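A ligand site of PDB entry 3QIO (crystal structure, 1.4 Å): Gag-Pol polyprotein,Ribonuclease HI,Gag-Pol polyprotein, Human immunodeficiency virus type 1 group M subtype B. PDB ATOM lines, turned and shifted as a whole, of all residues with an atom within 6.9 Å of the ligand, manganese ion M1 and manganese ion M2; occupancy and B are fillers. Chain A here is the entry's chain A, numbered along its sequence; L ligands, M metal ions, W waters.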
ATOM      1  N   VAL A  17      35.304   5.169   0.957  1.00  0.00           N
ATOM      2  CA  VAL A  17      34.413   4.947   2.100  1.00  0.00           C
ATOM      3  C   VAL A  17      33.724   6.240   2.503  1.00  0.00           C
ATOM      4  O   VAL A  17      34.238   7.329   2.267  1.00  0.00           O
ATOM      5  CB  VAL A  17      35.204   4.406   3.310  1.00  0.00           C
ATOM      6  CG1 VAL A  17      35.759   3.033   3.005  1.00  0.00           C
ATOM      7  CG2 VAL A  17      36.337   5.346   3.679  1.00  0.00           C
ATOM      8  N   ASP A  18      32.538   6.120   3.106  1.00  0.00           N
ATOM      9  CA  ASP A  18      31.863   7.284   3.673  1.00  0.00           C
ATOM     10  C   ASP A  18      30.749   6.833   4.602  1.00  0.00           C
ATOM     11  O   ASP A  18      30.321   5.678   4.558  1.00  0.00           O
ATOM     12  CB  ASP A  18      31.273   8.157   2.581  1.00  0.00           C
ATOM     13  CG  ASP A  18      30.985   9.577   3.052  1.00  0.00           C
ATOM     14  OD1 ASP A  18      31.582   9.999   4.056  1.00  0.00           O
ATOM     15  OD2 ASP A  18      30.192  10.263   2.383  1.00  0.00           O
ATOM     16  N   GLY A  19      30.298   7.759   5.444  1.00  0.00           N
ATOM     17  CA  GLY A  19      29.155   7.541   6.319  1.00  0.00           C
ATOM     18  C   GLY A  19      28.303   8.802   6.388  1.00  0.00           C
ATOM     19  O   GLY A  19      28.792   9.899   6.083  1.00  0.00           O
ATOM     20  N   ALA A  20      27.045   8.655   6.788  1.00  0.00           N
ATOM     21  CA  ALA A  20      26.150   9.783   7.010  1.00  0.00           C
ATOM     22  C   ALA A  20      25.283   9.452   8.196  1.00  0.00           C
ATOM     23  O   ALA A  20      24.867   8.310   8.336  1.00  0.00           O
ATOM     24  CB  ALA A  20      25.279  10.047   5.787  1.00  0.00           C
ATOM     25  N   ASN A  49      27.829  11.001  13.040  1.00  0.00           N
ATOM     26  CA  ASN A  49      28.629  11.162  11.833  1.00  0.00           C
ATOM     27  C   ASN A  49      30.010  10.506  11.959  1.00  0.00           C
ATOM     28  O   ASN A  49      30.412   9.745  11.096  1.00  0.00           O
ATOM     29  CB  ASN A  49      28.769  12.641  11.454  1.00  0.00           C
ATOM     30  CG  ASN A  49      27.559  13.167  10.696  1.00  0.00           C
ATOM     31  OD1 ASN A  49      27.013  12.482   9.820  1.00  0.00           O
ATOM     32  ND2 ASN A  49      27.139  14.387  11.024  1.00  0.00           N
ATOM     33  N   THR A  52      29.821   6.707  11.913  1.00  0.00           N
ATOM     34  CA  THR A  52      29.580   6.142  10.590  1.00  0.00           C
ATOM     35  C   THR A  52      30.845   6.121   9.720  1.00  0.00           C
ATOM     36  O   THR A  52      31.020   5.208   8.918  1.00  0.00           O
ATOM     37  CB  THR A  52      28.425   6.828   9.814  1.00  0.00           C
ATOM     38  OG1 THR A  52      28.766   8.177   9.508  1.00  0.00           O
ATOM     39  CG2 THR A  52      27.142   6.806  10.640  1.00  0.00           C
ATOM     40  N   GLU A  53      31.724   7.124   9.878  1.00  0.00           N
ATOM     41  CA  GLU A  53      32.978   7.115   9.122  1.00  0.00           C
ATOM     42  C   GLU A  53      33.858   5.937   9.557  1.00  0.00           C
ATOM     43  O   GLU A  53      34.483   5.281   8.715  1.00  0.00           O
ATOM     44  CB  GLU A  53      33.740   8.439   9.299  1.00  0.00           C
ATOM     45  CG  GLU A  53      32.996   9.700   8.896  1.00  0.00           C
ATOM     46  CD  GLU A  53      32.968   9.941   7.401  1.00  0.00           C
ATOM     47  OE1 GLU A  53      32.373  10.951   6.999  1.00  0.00           O
ATOM     48  OE2 GLU A  53      33.521   9.130   6.624  1.00  0.00           O
ATOM     49  N   THR A  72      39.305   8.087   2.267  1.00  0.00           N
ATOM     50  CA  THR A  72      38.312   8.595   3.204  1.00  0.00           C
ATOM     51  C   THR A  72      38.261  10.114   3.106  1.00  0.00           C
ATOM     52  O   THR A  72      39.239  10.731   2.659  1.00  0.00           O
ATOM     53  CB  THR A  72      38.698   8.198   4.645  1.00  0.00           C
ATOM     54  OG1 THR A  72      37.717   8.688   5.575  1.00  0.00           O
ATOM     55  CG2 THR A  72      40.046   8.778   5.031  1.00  0.00           C
ATOM     56  N   ASP A  73      37.133  10.711   3.494  1.00  0.00           N
ATOM     57  CA  ASP A  73      37.053  12.168   3.652  1.00  0.00           C
ATOM     58  C   ASP A  73      37.029  12.608   5.119  1.00  0.00           C
ATOM     59  O   ASP A  73      36.790  13.769   5.429  1.00  0.00           O
ATOM     60  CB  ASP A  73      35.882  12.790   2.845  1.00  0.00           C
ATOM     61  CG  ASP A  73      34.515  12.313   3.295  1.00  0.00           C
ATOM     62  OD1 ASP A  73      33.579  12.354   2.480  1.00  0.00           O
ATOM     63  OD2 ASP A  73      34.373  11.904   4.464  1.00  0.00           O
ATOM     64  N   SER A  74      37.311  11.669   6.014  1.00  0.00           N
ATOM     65  CA  SER A  74      37.308  11.919   7.451  1.00  0.00           C
ATOM     66  C   SER A  74      38.701  12.034   8.052  1.00  0.00           C
ATOM     67  O   SER A  74      39.399  11.031   8.227  1.00  0.00           O
ATOM     68  CB  SER A  74      36.548  10.784   8.159  1.00  0.00           C
ATOM     69  OG  SER A  74      36.585  10.953   9.566  1.00  0.00           O
ATOM     70  N   ALA A 127      35.527  16.223   1.289  1.00  0.00           N
ATOM     71  CA  ALA A 127      34.144  15.921   0.931  1.00  0.00           C
ATOM     72  C   ALA A 127      33.569  16.995   0.013  1.00  0.00           C
ATOM     73  O   ALA A 127      33.932  18.174   0.099  1.00  0.00           O
ATOM     74  CB  ALA A 127      33.290  15.796   2.183  1.00  0.00           C
ATOM     75  N   HIS A 128      32.659  16.571  -0.865  1.00  0.00           N
ATOM     76  CA  HIS A 128      31.922  17.479  -1.741  1.00  0.00           C
ATOM     77  C   HIS A 128      32.811  18.424  -2.539  1.00  0.00           C
ATOM     78  O   HIS A 128      32.556  19.625  -2.646  1.00  0.00           O
ATOM     79  CB  HIS A 128      30.844  18.210  -0.942  1.00  0.00           C
ATOM     80  CG  HIS A 128      29.857  17.273  -0.333  1.00  0.00           C
ATOM     81  ND1 HIS A 128      28.878  16.648  -1.070  1.00  0.00           N
ATOM     82  CD2 HIS A 128      29.755  16.776   0.927  1.00  0.00           C
ATOM     83  CE1 HIS A 128      28.188  15.847  -0.289  1.00  0.00           C
ATOM     84  NE2 HIS A 128      28.699  15.896   0.923  1.00  0.00           N
ATOM     85  N   LYS A 129      33.863  17.839  -3.119  1.00  0.00           N
ATOM     86  CA  LYS A 129      34.780  18.567  -3.984  1.00  0.00           C
ATOM     87  C   LYS A 129      34.867  17.911  -5.360  1.00  0.00           C
ATOM     88  O   LYS A 129      35.828  18.128  -6.101  1.00  0.00           O
ATOM     89  CB  LYS A 129      36.170  18.670  -3.356  1.00  0.00           C
ATOM     90  CG  LYS A 129      36.256  19.595  -2.161  1.00  0.00           C
ATOM     91  CD  LYS A 129      35.685  20.967  -2.487  1.00  0.00           C
ATOM     92  CE  LYS A 129      36.045  21.988  -1.415  1.00  0.00           C
ATOM     93  NZ  LYS A 129      37.435  22.475  -1.579  1.00  0.00           N
ATOM     94  N   ASN A 134      34.506   9.213  -4.143  1.00  0.00           N
ATOM     95  CA  ASN A 134      33.984   9.812  -2.928  1.00  0.00           C
ATOM     96  C   ASN A 134      32.553  10.324  -3.113  1.00  0.00           C
ATOM     97  O   ASN A 134      31.682  10.103  -2.262  1.00  0.00           O
ATOM     98  CB  ASN A 134      34.904  10.942  -2.461  1.00  0.00           C
ATOM     99  CG  ASN A 134      34.314  11.734  -1.318  1.00  0.00           C
ATOM    100  OD1 ASN A 134      33.734  12.799  -1.531  1.00  0.00           O
ATOM    101  ND2 ASN A 134      34.442  11.203  -0.100  1.00  0.00           N
ATOM    102  N   GLU A 135      32.291  11.012  -4.223  1.00  0.00           N
ATOM    103  CA  GLU A 135      30.932  11.474  -4.487  1.00  0.00           C
ATOM    104  C   GLU A 135      29.949  10.303  -4.665  1.00  0.00           C
ATOM    105  O   GLU A 135      28.806  10.376  -4.209  1.00  0.00           O
ATOM    106  CB  GLU A 135      30.893  12.429  -5.691  1.00  0.00           C
ATOM    107  CG  GLU A 135      31.648  13.748  -5.473  1.00  0.00           C
ATOM    108  CD  GLU A 135      30.935  14.738  -4.548  1.00  0.00           C
ATOM    109  OE1 GLU A 135      31.149  15.968  -4.743  1.00  0.00           O
ATOM    110  OE2 GLU A 135      30.187  14.337  -3.615  1.00  0.00           O
ATOM    111  N   VAL A 137      30.123   7.185  -3.276  1.00  0.00           N
ATOM    112  CA  VAL A 137      29.794   6.589  -1.985  1.00  0.00           C
ATOM    113  C   VAL A 137      28.967   7.554  -1.126  1.00  0.00           C
ATOM    114  O   VAL A 137      28.074   7.118  -0.395  1.00  0.00           O
ATOM    115  CB  VAL A 137      31.046   6.042  -1.229  1.00  0.00           C
ATOM    116  CG1 VAL A 137      32.015   7.159  -0.878  1.00  0.00           C
ATOM    117  CG2 VAL A 137      30.617   5.259   0.004  1.00  0.00           C
ATOM    118  N   ASP A 138      29.236   8.854  -1.233  1.00  0.00           N
ATOM    119  CA  ASP A 138      28.425   9.831  -0.507  1.00  0.00           C
ATOM    120  C   ASP A 138      26.954   9.747  -0.902  1.00  0.00           C
ATOM    121  O   ASP A 138      26.072   9.811  -0.039  1.00  0.00           O
ATOM    122  CB  ASP A 138      28.935  11.258  -0.717  1.00  0.00           C
ATOM    123  CG  ASP A 138      27.987  12.290  -0.111  1.00  0.00           C
ATOM    124  OD1 ASP A 138      28.086  12.516   1.104  1.00  0.00           O
ATOM    125  OD2 ASP A 138      27.147  12.835  -0.853  1.00  0.00           O
ATOM    126  N   LYS A 139      26.677   9.615  -2.189  1.00  0.00           N
ATOM    127  CA  LYS A 139      25.304   9.529  -2.661  1.00  0.00           C
ATOM    128  C   LYS A 139      24.632   8.289  -2.085  1.00  0.00           C
ATOM    129  O   LYS A 139      23.454   8.337  -1.687  1.00  0.00           O
ATOM    130  CB  LYS A 139      25.263   9.510  -4.191  1.00  0.00           C
ATOM    131  CG  LYS A 139      23.879   9.313  -4.777  1.00  0.00           C
ATOM    132  CD  LYS A 139      23.946   9.207  -6.297  1.00  0.00           C
ATOM    133  CE  LYS A 139      22.561   9.209  -6.928  1.00  0.00           C
ATOM    134  NZ  LYS A 139      22.634   9.145  -8.421  1.00  0.00           N
ATOM    135  N   VAL A 141      25.378   6.571   0.797  1.00  0.00           N
ATOM    136  CA  VAL A 141      25.149   6.579   2.244  1.00  0.00           C
ATOM    137  C   VAL A 141      24.263   7.726   2.735  1.00  0.00           C
ATOM    138  O   VAL A 141      23.663   7.642   3.812  1.00  0.00           O
ATOM    139  CB  VAL A 141      26.479   6.564   3.059  1.00  0.00           C
ATOM    140  CG1 VAL A 141      27.304   5.333   2.714  1.00  0.00           C
ATOM    141  CG2 VAL A 141      27.271   7.836   2.810  1.00  0.00           C
ATOM    142  N   SER A 142      24.150   8.793   1.955  1.00  0.00           N
ATOM    143  CA  SER A 142      23.403   9.978   2.374  1.00  0.00           C
ATOM    144  C   SER A 142      21.925   9.890   2.021  1.00  0.00           C
ATOM    145  O   SER A 142      21.090  10.590   2.600  1.00  0.00           O
ATOM    146  CB  SER A 142      24.018  11.237   1.761  1.00  0.00           C
ATOM    147  OG  SER A 142      25.344  11.435   2.228  1.00  0.00           O
ATOM    148  N   ARG A 146      20.527  12.429   4.709  1.00  0.00           N
ATOM    149  CA  ARG A 146      20.787  13.854   4.533  1.00  0.00           C
ATOM    150  C   ARG A 146      19.970  14.408   3.363  1.00  0.00           C
ATOM    151  O   ARG A 146      19.939  13.810   2.290  1.00  0.00           O
ATOM    152  CB  ARG A 146      22.285  14.095   4.263  1.00  0.00           C
ATOM    153  CG  ARG A 146      22.686  15.567   4.254  1.00  0.00           C
ATOM    154  CD  ARG A 146      24.141  15.737   3.768  1.00  0.00           C
ATOM    155  NE  ARG A 146      24.248  15.481   2.334  1.00  0.00           N
ATOM    156  CZ  ARG A 146      25.184  14.711   1.779  1.00  0.00           C
ATOM    157  NH1 ARG A 146      26.084  14.119   2.535  1.00  0.00           N
ATOM    158  NH2 ARG A 146      25.199  14.530   0.459  1.00  0.00           N
ATOM    159  N   LYS A 147      19.283  15.525   3.591  1.00  0.00           N
ATOM    160  CA  LYS A 147      18.424  16.102   2.568  1.00  0.00           C
ATOM    161  C   LYS A 147      19.250  16.598   1.391  1.00  0.00           C
ATOM    162  O   LYS A 147      20.319  17.182   1.577  1.00  0.00           O
ATOM    163  CB  LYS A 147      17.599  17.247   3.164  1.00  0.00           C
ATOM    164  CG  LYS A 147      16.530  17.778   2.214  1.00  0.00           C
ATOM    165  CD  LYS A 147      15.609  18.759   2.929  1.00  0.00           C
ATOM    166  CE  LYS A 147      14.416  19.121   2.056  1.00  0.00           C
ATOM    167  NZ  LYS A 147      13.411  19.935   2.798  1.00  0.00           N
ATOM    168  N   VAL A 148      18.748  16.354   0.183  1.00  0.00           N
ATOM    169  CA  VAL A 148      19.438  16.798  -1.031  1.00  0.00           C
ATOM    170  C   VAL A 148      19.418  18.327  -1.151  1.00  0.00           C
ATOM    171  O   VAL A 148      20.372  18.939  -1.616  1.00  0.00           O
ATOM    172  CB  VAL A 148      18.793  16.192  -2.284  1.00  0.00           C
ATOM    173  CG1 VAL A 148      19.508  16.685  -3.532  1.00  0.00           C
ATOM    174  CG2 VAL A 148      18.833  14.671  -2.203  1.00  0.00           C
HETATM  175  C1  LIG L   1      28.631  18.502   4.246  1.00  0.00           C
HETATM  176  C2  LIG L   1      29.625  19.046   5.007  1.00  0.00           C
HETATM  177  C3  LIG L   1      30.669  18.236   5.485  1.00  0.00           C
HETATM  178  C4  LIG L   1      30.654  16.836   5.179  1.00  0.00           C
HETATM  179  C5  LIG L   1      29.614  16.281   4.402  1.00  0.00           C
HETATM  180  C6  LIG L   1      28.596  17.055   3.947  1.00  0.00           C
HETATM  181  C7  LIG L   1      29.620  14.805   4.078  1.00  0.00           C
HETATM  182  N1  LIG L   1      31.738  15.993   5.682  1.00  0.00           N
HETATM  183  N2  LIG L   1      30.683  13.999   4.566  1.00  0.00           N
HETATM  184  O1  LIG L   1      28.752  14.309   3.372  1.00  0.00           O
HETATM  185  C8  LIG L   1      31.746  14.578   5.385  1.00  0.00           C
HETATM  186  O2  LIG L   1      32.628  13.855   5.793  1.00  0.00           O
HETATM  187  O3  LIG L   1      30.667  12.740   4.317  1.00  0.00           O
HETATM  188  S1  LIG L   1      27.319  19.507   3.698  1.00  0.00           S
HETATM  189  C9  LIG L   1      27.627  19.862   2.012  1.00  0.00           C
HETATM  190  O4  LIG L   1      26.055  18.834   3.894  1.00  0.00           O
HETATM  191  O5  LIG L   1      27.229  20.699   4.520  1.00  0.00           O
HETATM  192  C10 LIG L   1      26.862  19.230   1.060  1.00  0.00           C
HETATM  193  C11 LIG L   1      27.082  19.504  -0.303  1.00  0.00           C
HETATM  194  C12 LIG L   1      28.081  20.454  -0.691  1.00  0.00           C
HETATM  195  C13 LIG L   1      28.856  21.117   0.288  1.00  0.00           C
HETATM  196  C14 LIG L   1      28.649  20.848   1.617  1.00  0.00           C
HETATM  197 MN    MN M   1      32.394  11.744   5.047  1.00  0.00          MN
HETATM  198 MN    MN M   2      29.425  12.263   2.712  1.00  0.00          MN
HETATM  199  O   HOH W   1      34.608  14.376   7.466  1.00  0.00           O
HETATM  200  O   HOH W   2      24.615  18.533   6.635  1.00  0.00           O
HETATM  201  O   HOH W   3      27.854  11.482   4.034  1.00  0.00           O
HETATM  202  O   HOH W   4      26.625  13.500   5.518  1.00  0.00           O
HETATM  203  O   HOH W   5      31.077  13.096   1.561  1.00  0.00           O
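Residues that only touch the ligand: Gly 19 (3.8 Å) and Ala 127 (3.8 Å).
Hydrophobic or aromatic side chains within 4 Å of the ligand: Ala 127 and His 128.
The nearest printed residue that does not touch the ligand is Ser 142 (4.6 Å).
Water W3 bridges the backbone carbonyl oxygen (O) of Gly 19 (2.8 Å) and the side-chain hydroxyl (OG) of Ser 142 (3.1 Å).
Residues that only touch manganese ion M2: Arg 146 (3.8 Å).
Three residues have an atom within 4 Å of manganese ion M2: Asp 18, Asp 138 and Arg 146.
The nearest printed residue that does not touch manganese ion M2 is His 128 (4.1 Å).
The guanidinium group (NH1) of Arg 146 lies close to an oxygen (O1) of the ligand (2.8 Å).
NE2 of His 128 sits close to O1 of the ligand (2.9 Å).
O3 of the ligand is bound to manganese ion M2, 2.1 Å away.
The side-chain carboxylate (OD1) of Asp 138 is bound to manganese ion M2 (2.1 Å).
OD2 of Asp 18 is bound to manganese ion M2 (2.2 Å).
Water W5 is bound to manganese ion M2 (2.2 Å).
Water W3 is bound to manganese ion M2, 2.2 Å away.
O1 of the ligand binds manganese ion M2 (2.3 Å).
Manganese ion M2 has six donor atoms within binding distance.
OG of Ser 142 is in hydrogen-bond range of NH1 of Arg 146 (2.8 Å).
O of Asp 138 sits at hydrogen-bond distance from OG of Ser 142 (2.9 Å).
A ring nitrogen (NE2) of His 128 sits close to the side-chain carboxylate (OD1) of Asp 138 (3.4 Å).
The side-chain carboxylate of Asp 73 sits at hydrogen-bond distance from the side-chain amide nitrogen of Asn 134 (3.0 Å).
OD2 of Asp 138 lies within salt-bridge range of NH2 of Arg 146, 2.9 Å away.
Manganese ion M1 is bound by the side-chain carboxylate (OD2) of Asp 73 (2.1 Å), the side-chain carboxylate (OE1) of Glu 53 (2.1 Å), an oxygen (O3) of the ligand (2.1 Å), the side-chain carboxylate (OD1) of Asp 18 (2.2 Å) and an oxygen (O2) of the ligand (2.3 Å).
Slightly farther from manganese ion M1 lies OD1 of Asp 73 (2.9 Å).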
